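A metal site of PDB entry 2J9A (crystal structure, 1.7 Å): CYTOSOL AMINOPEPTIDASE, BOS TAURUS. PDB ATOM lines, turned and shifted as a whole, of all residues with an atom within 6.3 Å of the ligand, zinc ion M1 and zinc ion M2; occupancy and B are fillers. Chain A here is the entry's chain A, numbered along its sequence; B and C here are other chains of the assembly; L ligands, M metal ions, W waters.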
ATOM      1  N   LYS A 250      28.284 -15.097  13.856  1.00  0.00           N
ATOM      2  CA  LYS A 250      27.247 -14.820  14.840  1.00  0.00           C
ATOM      3  C   LYS A 250      27.064 -13.293  15.044  1.00  0.00           C
ATOM      4  O   LYS A 250      28.032 -12.610  15.384  1.00  0.00           O
ATOM      5  CB  LYS A 250      27.637 -15.508  16.165  1.00  0.00           C
ATOM      6  CG  LYS A 250      26.775 -15.075  17.382  1.00  0.00           C
ATOM      7  CD  LYS A 250      27.352 -15.778  18.695  1.00  0.00           C
ATOM      8  CE  LYS A 250      26.601 -15.223  19.914  1.00  0.00           C
ATOM      9  NZ  LYS A 250      27.222 -15.676  21.202  1.00  0.00           N
ATOM     10  N   ILE A 252      25.000 -11.449  17.254  1.00  0.00           N
ATOM     11  CA  ILE A 252      24.131 -11.025  18.351  1.00  0.00           C
ATOM     12  C   ILE A 252      24.562  -9.594  18.752  1.00  0.00           C
ATOM     13  O   ILE A 252      25.643  -9.388  19.322  1.00  0.00           O
ATOM     14  CB  ILE A 252      24.284 -12.006  19.537  1.00  0.00           C
ATOM     15  CG1 ILE A 252      23.665 -13.364  19.136  1.00  0.00           C
ATOM     16  CG2 ILE A 252      23.589 -11.415  20.796  1.00  0.00           C
ATOM     17  CD1 ILE A 252      22.108 -13.304  18.874  1.00  0.00           C
ATOM     18  N   ASP A 255      23.863  -9.344  23.881  1.00  0.00           N
ATOM     19  CA  ASP A 255      23.452 -10.608  24.560  1.00  0.00           C
ATOM     20  C   ASP A 255      23.241 -10.349  26.076  1.00  0.00           C
ATOM     21  O   ASP A 255      24.195 -10.238  26.858  1.00  0.00           O
ATOM     22  CB  ASP A 255      24.524 -11.688  24.370  1.00  0.00           C
ATOM     23  CG  ASP A 255      24.076 -13.062  24.872  1.00  0.00           C
ATOM     24  OD1 ASP A 255      22.877 -13.198  25.176  1.00  0.00           O
ATOM     25  OD2 ASP A 255      24.936 -13.959  24.906  1.00  0.00           O
ATOM     26  N   SER A 256      21.962 -10.241  26.477  1.00  0.00           N
ATOM     27  CA  SER A 256      21.622 -10.151  27.906  1.00  0.00           C
ATOM     28  C   SER A 256      21.564 -11.561  28.529  1.00  0.00           C
ATOM     29  O   SER A 256      21.372 -11.686  29.766  1.00  0.00           O
ATOM     30  CB  SER A 256      20.237  -9.490  28.115  1.00  0.00           C
ATOM     31  OG  SER A 256      19.224 -10.381  27.609  1.00  0.00           O
ATOM     32  N   GLY A 257      21.681 -12.576  27.689  1.00  0.00           N
ATOM     33  CA  GLY A 257      21.338 -13.964  28.077  1.00  0.00           C
ATOM     34  C   GLY A 257      19.883 -14.355  27.840  1.00  0.00           C
ATOM     35  O   GLY A 257      19.567 -15.559  27.756  1.00  0.00           O
ATOM     36  N   LYS A 262      22.080 -13.024  32.161  1.00  0.00           N
ATOM     37  CA  LYS A 262      23.472 -12.894  32.665  1.00  0.00           C
ATOM     38  C   LYS A 262      23.509 -12.042  33.930  1.00  0.00           C
ATOM     39  O   LYS A 262      22.612 -11.246  34.165  1.00  0.00           O
ATOM     40  CB  LYS A 262      24.335 -12.183  31.602  1.00  0.00           C
ATOM     41  CG  LYS A 262      24.587 -13.108  30.387  1.00  0.00           C
ATOM     42  CD  LYS A 262      25.370 -12.352  29.323  1.00  0.00           C
ATOM     43  CE  LYS A 262      25.715 -13.239  28.081  1.00  0.00           C
ATOM     44  NZ  LYS A 262      26.428 -14.542  28.477  1.00  0.00           N
ATOM     45  N   LEU A 269      30.129  -5.708  27.923  1.00  0.00           N
ATOM     46  CA  LEU A 269      31.012  -6.267  26.844  1.00  0.00           C
ATOM     47  C   LEU A 269      30.209  -7.078  25.823  1.00  0.00           C
ATOM     48  O   LEU A 269      30.718  -7.342  24.705  1.00  0.00           O
ATOM     49  CB  LEU A 269      32.085  -7.173  27.438  1.00  0.00           C
ATOM     50  CG  LEU A 269      33.063  -6.384  28.347  1.00  0.00           C
ATOM     51  CD1 LEU A 269      34.034  -7.428  28.966  1.00  0.00           C
ATOM     52  CD2 LEU A 269      33.827  -5.277  27.591  1.00  0.00           C
ATOM     53  N   MET A 270      28.984  -7.453  26.188  1.00  0.00           N
ATOM     54  CA  MET A 270      28.139  -8.238  25.284  1.00  0.00           C
ATOM     55  C   MET A 270      27.629  -7.422  24.090  1.00  0.00           C
ATOM     56  O   MET A 270      26.995  -7.983  23.191  1.00  0.00           O
ATOM     57  CB  MET A 270      26.967  -8.914  26.021  1.00  0.00           C
ATOM     58  CG  MET A 270      27.434 -10.021  27.034  1.00  0.00           C
ATOM     59  SD  MET A 270      28.416 -11.336  26.192  1.00  0.00           S
ATOM     60  CE  MET A 270      30.113 -10.774  26.374  1.00  0.00           C
ATOM     61  N   ASP A 273      29.007  -9.115  21.036  1.00  0.00           N
ATOM     62  CA  ASP A 273      28.576 -10.487  20.728  1.00  0.00           C
ATOM     63  C   ASP A 273      28.222 -10.640  19.260  1.00  0.00           C
ATOM     64  O   ASP A 273      27.774 -11.704  18.868  1.00  0.00           O
ATOM     65  CB  ASP A 273      27.399 -10.892  21.592  1.00  0.00           C
ATOM     66  CG  ASP A 273      27.361 -12.401  21.850  1.00  0.00           C
ATOM     67  OD1 ASP A 273      28.411 -13.063  21.749  1.00  0.00           O
ATOM     68  OD2 ASP A 273      26.250 -12.841  22.170  1.00  0.00           O
ATOM     69  N   ASN A 305      19.460 -10.500  21.983  1.00  0.00           N
ATOM     70  CA  ASN A 305      18.975 -11.580  22.870  1.00  0.00           C
ATOM     71  C   ASN A 305      18.510 -10.923  24.164  1.00  0.00           C
ATOM     72  O   ASN A 305      19.346 -10.572  25.016  1.00  0.00           O
ATOM     73  CB  ASN A 305      20.082 -12.650  23.138  1.00  0.00           C
ATOM     74  CG  ASN A 305      19.526 -13.900  23.848  1.00  0.00           C
ATOM     75  OD1 ASN A 305      18.329 -14.241  23.702  1.00  0.00           O
ATOM     76  ND2 ASN A 305      20.397 -14.620  24.567  1.00  0.00           N
ATOM     77  N   THR A 331      18.745 -20.166  27.441  1.00  0.00           N
ATOM     78  CA  THR A 331      18.499 -19.153  26.383  1.00  0.00           C
ATOM     79  C   THR A 331      19.743 -18.303  26.113  1.00  0.00           C
ATOM     80  O   THR A 331      19.737 -17.496  25.154  1.00  0.00           O
ATOM     81  CB  THR A 331      17.326 -18.197  26.725  1.00  0.00           C
ATOM     82  OG1 THR A 331      17.678 -17.378  27.869  1.00  0.00           O
ATOM     83  CG2 THR A 331      16.029 -18.970  27.015  1.00  0.00           C
ATOM     84  N   ASP A 332      20.783 -18.473  26.924  1.00  0.00           N
ATOM     85  CA  ASP A 332      22.031 -17.728  26.744  1.00  0.00           C
ATOM     86  C   ASP A 332      23.025 -18.521  25.864  1.00  0.00           C
ATOM     87  O   ASP A 332      24.096 -18.034  25.534  1.00  0.00           O
ATOM     88  CB  ASP A 332      22.646 -17.437  28.120  1.00  0.00           C
ATOM     89  CG  ASP A 332      23.767 -16.398  28.111  1.00  0.00           C
ATOM     90  OD1 ASP A 332      24.029 -15.699  27.082  1.00  0.00           O
ATOM     91  OD2 ASP A 332      24.403 -16.285  29.198  1.00  0.00           O
ATOM     92  N   ALA A 333      22.614 -19.733  25.474  1.00  0.00           N
ATOM     93  CA  ALA A 333      23.349 -20.471  24.443  1.00  0.00           C
ATOM     94  C   ALA A 333      22.656 -20.163  23.086  1.00  0.00           C
ATOM     95  O   ALA A 333      22.217 -21.064  22.364  1.00  0.00           O
ATOM     96  CB  ALA A 333      23.357 -22.005  24.746  1.00  0.00           C
ATOM     97  N   GLU A 334      22.526 -18.870  22.799  1.00  0.00           N
ATOM     98  CA  GLU A 334      21.739 -18.412  21.651  1.00  0.00           C
ATOM     99  C   GLU A 334      22.571 -18.379  20.376  1.00  0.00           C
ATOM    100  O   GLU A 334      21.999 -18.494  19.285  1.00  0.00           O
ATOM    101  CB  GLU A 334      21.125 -17.017  21.923  1.00  0.00           C
ATOM    102  CG  GLU A 334      22.095 -15.791  21.638  1.00  0.00           C
ATOM    103  CD  GLU A 334      23.295 -15.692  22.623  1.00  0.00           C
ATOM    104  OE1 GLU A 334      23.147 -16.155  23.777  1.00  0.00           O
ATOM    105  OE2 GLU A 334      24.334 -15.130  22.261  1.00  0.00           O
ATOM    106  N   GLY A 335      23.875 -18.204  20.490  1.00  0.00           N
ATOM    107  CA  GLY A 335      24.735 -18.187  19.270  1.00  0.00           C
ATOM    108  C   GLY A 335      24.623 -19.461  18.468  1.00  0.00           C
ATOM    109  O   GLY A 335      24.529 -19.461  17.205  1.00  0.00           O
ATOM    110  N   THR A 359      31.603 -15.321  18.950  1.00  0.00           N
ATOM    111  CA  THR A 359      32.016 -15.087  20.359  1.00  0.00           C
ATOM    112  C   THR A 359      31.165 -16.073  21.209  1.00  0.00           C
ATOM    113  O   THR A 359      30.211 -15.676  21.857  1.00  0.00           O
ATOM    114  CB  THR A 359      31.745 -13.622  20.738  1.00  0.00           C
ATOM    115  OG1 THR A 359      30.456 -13.259  20.224  1.00  0.00           O
ATOM    116  CG2 THR A 359      32.829 -12.663  20.127  1.00  0.00           C
ATOM    117  N   LEU A 360      31.456 -17.372  21.116  1.00  0.00           N
ATOM    118  CA  LEU A 360      30.398 -18.352  21.371  1.00  0.00           C
ATOM    119  C   LEU A 360      30.268 -18.785  22.844  1.00  0.00           C
ATOM    120  O   LEU A 360      29.171 -19.036  23.302  1.00  0.00           O
ATOM    121  CB  LEU A 360      30.554 -19.598  20.452  1.00  0.00           C
ATOM    122  CG  LEU A 360      29.274 -20.445  20.271  1.00  0.00           C
ATOM    123  CD1 LEU A 360      28.129 -19.659  19.622  1.00  0.00           C
ATOM    124  CD2 LEU A 360      29.591 -21.758  19.474  1.00  0.00           C
ATOM    125  N   THR A 361      31.411 -18.982  23.506  1.00  0.00           N
ATOM    126  CA  THR A 361      31.322 -19.579  24.831  1.00  0.00           C
ATOM    127  C   THR A 361      32.244 -18.940  25.819  1.00  0.00           C
ATOM    128  O   THR A 361      33.370 -18.600  25.488  1.00  0.00           O
ATOM    129  CB  THR A 361      31.623 -21.137  24.781  1.00  0.00           C
ATOM    130  OG1 THR A 361      32.975 -21.389  24.393  1.00  0.00           O
ATOM    131  CG2 THR A 361      30.689 -21.896  23.799  1.00  0.00           C
ATOM    132  N   GLY A 362      31.794 -18.835  27.078  1.00  0.00           N
ATOM    133  CA  GLY A 362      32.694 -18.447  28.160  1.00  0.00           C
ATOM    134  C   GLY A 362      33.763 -19.497  28.326  1.00  0.00           C
ATOM    135  O   GLY A 362      34.919 -19.163  28.709  1.00  0.00           O
ATOM    136  N   ALA A 363      33.430 -20.741  28.007  1.00  0.00           N
ATOM    137  CA  ALA A 363      34.377 -21.848  28.187  1.00  0.00           C
ATOM    138  C   ALA A 363      35.628 -21.657  27.327  1.00  0.00           C
ATOM    139  O   ALA A 363      36.756 -21.999  27.724  1.00  0.00           O
ATOM    140  CB  ALA A 363      33.719 -23.170  27.846  1.00  0.00           C
ATOM    141  N   ASP A 365      37.080 -18.811  26.628  1.00  0.00           N
ATOM    142  CA  ASP A 365      37.932 -17.871  27.337  1.00  0.00           C
ATOM    143  C   ASP A 365      38.644 -18.574  28.499  1.00  0.00           C
ATOM    144  O   ASP A 365      39.839 -18.392  28.727  1.00  0.00           O
ATOM    145  CB  ASP A 365      37.104 -16.706  27.910  1.00  0.00           C
ATOM    146  CG  ASP A 365      37.991 -15.717  28.596  1.00  0.00           C
ATOM    147  OD1 ASP A 365      38.890 -15.195  27.909  1.00  0.00           O
ATOM    148  OD2 ASP A 365      37.916 -15.621  29.822  1.00  0.00           O
ATOM    149  N   ALA A 451      35.436 -15.997  21.489  1.00  0.00           N
ATOM    150  CA  ALA A 451      35.058 -15.356  22.763  1.00  0.00           C
ATOM    151  C   ALA A 451      36.277 -14.902  23.577  1.00  0.00           C
ATOM    152  O   ALA A 451      36.258 -13.832  24.213  1.00  0.00           O
ATOM    153  CB  ALA A 451      34.166 -16.318  23.637  1.00  0.00           C
ATOM    154  N   GLY A 452      37.352 -15.693  23.578  1.00  0.00           N
ATOM    155  CA  GLY A 452      38.541 -15.315  24.364  1.00  0.00           C
ATOM    156  C   GLY A 452      39.369 -14.162  23.768  1.00  0.00           C
ATOM    157  O   GLY A 452      40.085 -13.489  24.480  1.00  0.00           O
ATOM    158  N   MET A 454      37.933 -11.621  22.110  1.00  0.00           N
ATOM    159  CA  MET A 454      36.994 -10.507  21.880  1.00  0.00           C
ATOM    160  C   MET A 454      37.567  -9.146  22.313  1.00  0.00           C
ATOM    161  O   MET A 454      37.311  -8.121  21.653  1.00  0.00           O
ATOM    162  CB  MET A 454      35.681 -10.779  22.651  1.00  0.00           C
ATOM    163  CG  MET A 454      34.420 -10.133  22.085  1.00  0.00           C
ATOM    164  SD  MET A 454      32.991 -10.587  23.114  1.00  0.00           S
ATOM    165  CE  MET A 454      33.529  -9.857  24.675  1.00  0.00           C
ATOM    166  N   THR A 455      38.313  -9.142  23.411  1.00  0.00           N
ATOM    167  CA  THR A 455      38.865  -7.894  23.970  1.00  0.00           C
ATOM    168  C   THR A 455      40.391  -7.973  24.085  1.00  0.00           C
ATOM    169  O   THR A 455      40.990  -9.068  24.025  1.00  0.00           O
ATOM    170  CB  THR A 455      38.310  -7.610  25.404  1.00  0.00           C
ATOM    171  OG1 THR A 455      38.852  -8.600  26.301  1.00  0.00           O
ATOM    172  CG2 THR A 455      36.796  -7.686  25.434  1.00  0.00           C
ATOM    173  N   ALA B   1      27.354 -18.854  25.733  1.00  0.00           N
ATOM    174  CA  ALA B   1      26.961 -19.858  26.708  1.00  0.00           C
ATOM    175  C   ALA B   1      27.860 -19.791  27.932  1.00  0.00           C
ATOM    176  O   ALA B   1      29.070 -19.670  27.760  1.00  0.00           O
ATOM    177  CB  ALA B   1      27.033 -21.282  26.095  1.00  0.00           C
ATOM    178  N   MLE B   2      27.246 -19.904  29.126  1.00  0.00           N
ATOM    179  CN  MLE B   2      25.777 -20.074  29.165  1.00  0.00           C
ATOM    180  CA  MLE B   2      28.092 -19.875  30.367  1.00  0.00           C
ATOM    181  CB  MLE B   2      27.596 -18.813  31.340  1.00  0.00           C
ATOM    182  CG  MLE B   2      27.679 -17.407  30.658  1.00  0.00           C
ATOM    183  CD1 MLE B   2      27.286 -16.312  31.653  1.00  0.00           C
ATOM    184  CD2 MLE B   2      29.063 -17.081  30.076  1.00  0.00           C
ATOM    185  C   MLE B   2      28.277 -21.346  30.894  1.00  0.00           C
ATOM    186  O   MLE B   2      27.622 -22.269  30.378  1.00  0.00           O
ATOM    187  N   ARG C 425      41.120 -14.564  35.188  1.00  0.00           N
ATOM    188  CA  ARG C 425      40.519 -15.879  35.205  1.00  0.00           C
ATOM    189  C   ARG C 425      40.778 -16.671  33.922  1.00  0.00           C
ATOM    190  O   ARG C 425      40.759 -17.906  33.901  1.00  0.00           O
ATOM    191  CB  ARG C 425      38.998 -15.832  35.479  1.00  0.00           C
ATOM    192  CG  ARG C 425      38.205 -14.965  34.462  1.00  0.00           C
ATOM    193  CD  ARG C 425      36.942 -15.667  33.871  1.00  0.00           C
ATOM    194  NE  ARG C 425      36.587 -15.091  32.555  1.00  0.00           N
ATOM    195  CZ  ARG C 425      35.591 -15.500  31.755  1.00  0.00           C
ATOM    196  NH1 ARG C 425      35.387 -14.882  30.599  1.00  0.00           N
ATOM    197  NH2 ARG C 425      34.789 -16.499  32.091  1.00  0.00           N
ATOM    198  N   SER C 426      41.123 -15.963  32.858  1.00  0.00           N
ATOM    199  CA  SER C 426      41.150 -16.610  31.537  1.00  0.00           C
ATOM    200  C   SER C 426      42.331 -17.556  31.421  1.00  0.00           C
ATOM    201  O   SER C 426      43.392 -17.280  31.958  1.00  0.00           O
ATOM    202  CB  SER C 426      41.321 -15.525  30.480  1.00  0.00           C
ATOM    203  OG  SER C 426      40.260 -14.579  30.645  1.00  0.00           O
HETATM  204  C1  LIG L   1      34.907 -11.852  28.179  1.00  0.00           C
HETATM  205  C2  LIG L   1      35.136 -13.161  27.396  1.00  0.00           C
HETATM  206  C3  LIG L   1      34.018 -14.222  27.602  1.00  0.00           C
HETATM  207  C4  LIG L   1      32.681 -13.786  26.980  1.00  0.00           C
HETATM  208  C5  LIG L   1      31.808 -15.031  26.670  1.00  0.00           C
HETATM  209  C6  LIG L   1      30.469 -14.595  26.033  1.00  0.00           C
HETATM  210  C7  LIG L   1      29.668 -15.791  25.556  1.00  0.00           C
HETATM  211  C8  LIG L   1      28.213 -15.399  25.196  1.00  0.00           C
HETATM  212  N1  LIG L   1      28.187 -14.480  24.000  1.00  0.00           N
HETATM  213  C9  LIG L   1      27.457 -16.667  24.785  1.00  0.00           C
HETATM  214  O1  LIG L   1      26.176 -16.365  24.291  1.00  0.00           O
HETATM  215  C10 LIG L   1      27.150 -17.579  25.968  1.00  0.00           C
HETATM  216  O2  LIG L   1      26.738 -17.095  27.021  1.00  0.00           O
HETATM  217 ZN    ZN M   1      24.521 -15.918  25.228  1.00  0.00          ZN
HETATM  218 ZN    ZN M   2      26.308 -14.732  22.895  1.00  0.00          ZN
HETATM  219  O   HOH W   1      25.881 -18.106  22.327  1.00  0.00           O
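Four residues have an atom within 4 Å of zinc ion M2: Lys 250, Asp 255, Asp 273 and Glu 334.
A carbon (C10) of the ligand is covalently linked to the backbone NH (N) of Ala 1 of chain B, 1.3 Å away.
An oxygen (O2) of the ligand is in hydrogen-bond range of the side-chain amino group (NZ) of Lys 262.
The backbone carbonyl oxygen (O) of Thr 359 lies close to a nitrogen (N1) of the ligand (3.2 Å).
Residues that only touch the ligand: Leu 360, Arg 425 of chain C, Ala 451, MLE 2 of chain B, Gly 362, Met 270 and Asp 365.
Hydrophobic or aromatic side chains within 4 Å of the ligand: Met 270 and Ala 1 of chain B.
The backbone carbonyl oxygen of Asp 332 sits close to the backbone NH of Ala 1 of chain B (3.4 Å).
The backbone NH (N) of Ala 1 of chain B lies within hydrogen-bond range of the backbone carbonyl oxygen (O) of Leu 360, 3.0 Å away.
The backbone carbonyl oxygen (O) of Asp 273 sits at hydrogen-bond distance from the backbone NH (N) of Ile 252, 3.2 Å away.
OD2 of Asp 255 lies close to NZ of Lys 262 (3.9 Å).
The backbone NH (N) of Asp 255 is in hydrogen-bond range of the backbone carbonyl oxygen (O) of Met 270.
NZ of Lys 250 lies close to O of Thr 359, 3.1 Å away.
OD2 of Asp 365 lies within salt-bridge range of NH1 of Arg 425 of chain C, at 2.7 Å.
OG of Ser 426 of chain C lies within hydrogen-bond range of OD2 of Asp 365 (2.7 Å).
Zinc ion M1 is bound by the side-chain carboxylate of Asp 332, an oxygen (O1) of the ligand, the side-chain carboxylate of Glu 334, the side-chain carboxylate of Asp 255 and the backbone carbonyl oxygen of Asp 332.
Zinc ion M1 has five donor atoms within binding distance.
Zinc ion M2 is bound by OD2 of Asp 273 (2.0 Å).
OE2 of Glu 334 binds zinc ion M2, at 2.1 Å.
NZ of Lys 250 is bound to zinc ion M2.
An oxygen (O1) of the ligand binds zinc ion M2 (2.2 Å).
Zinc ion M2 is bound by N1 of the ligand, 2.2 Å away.
OD2 of Asp 255 binds zinc ion M2.
Three residues have an atom within 4 Å of zinc ion M1: Asp 255, Asp 332 and Glu 334.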
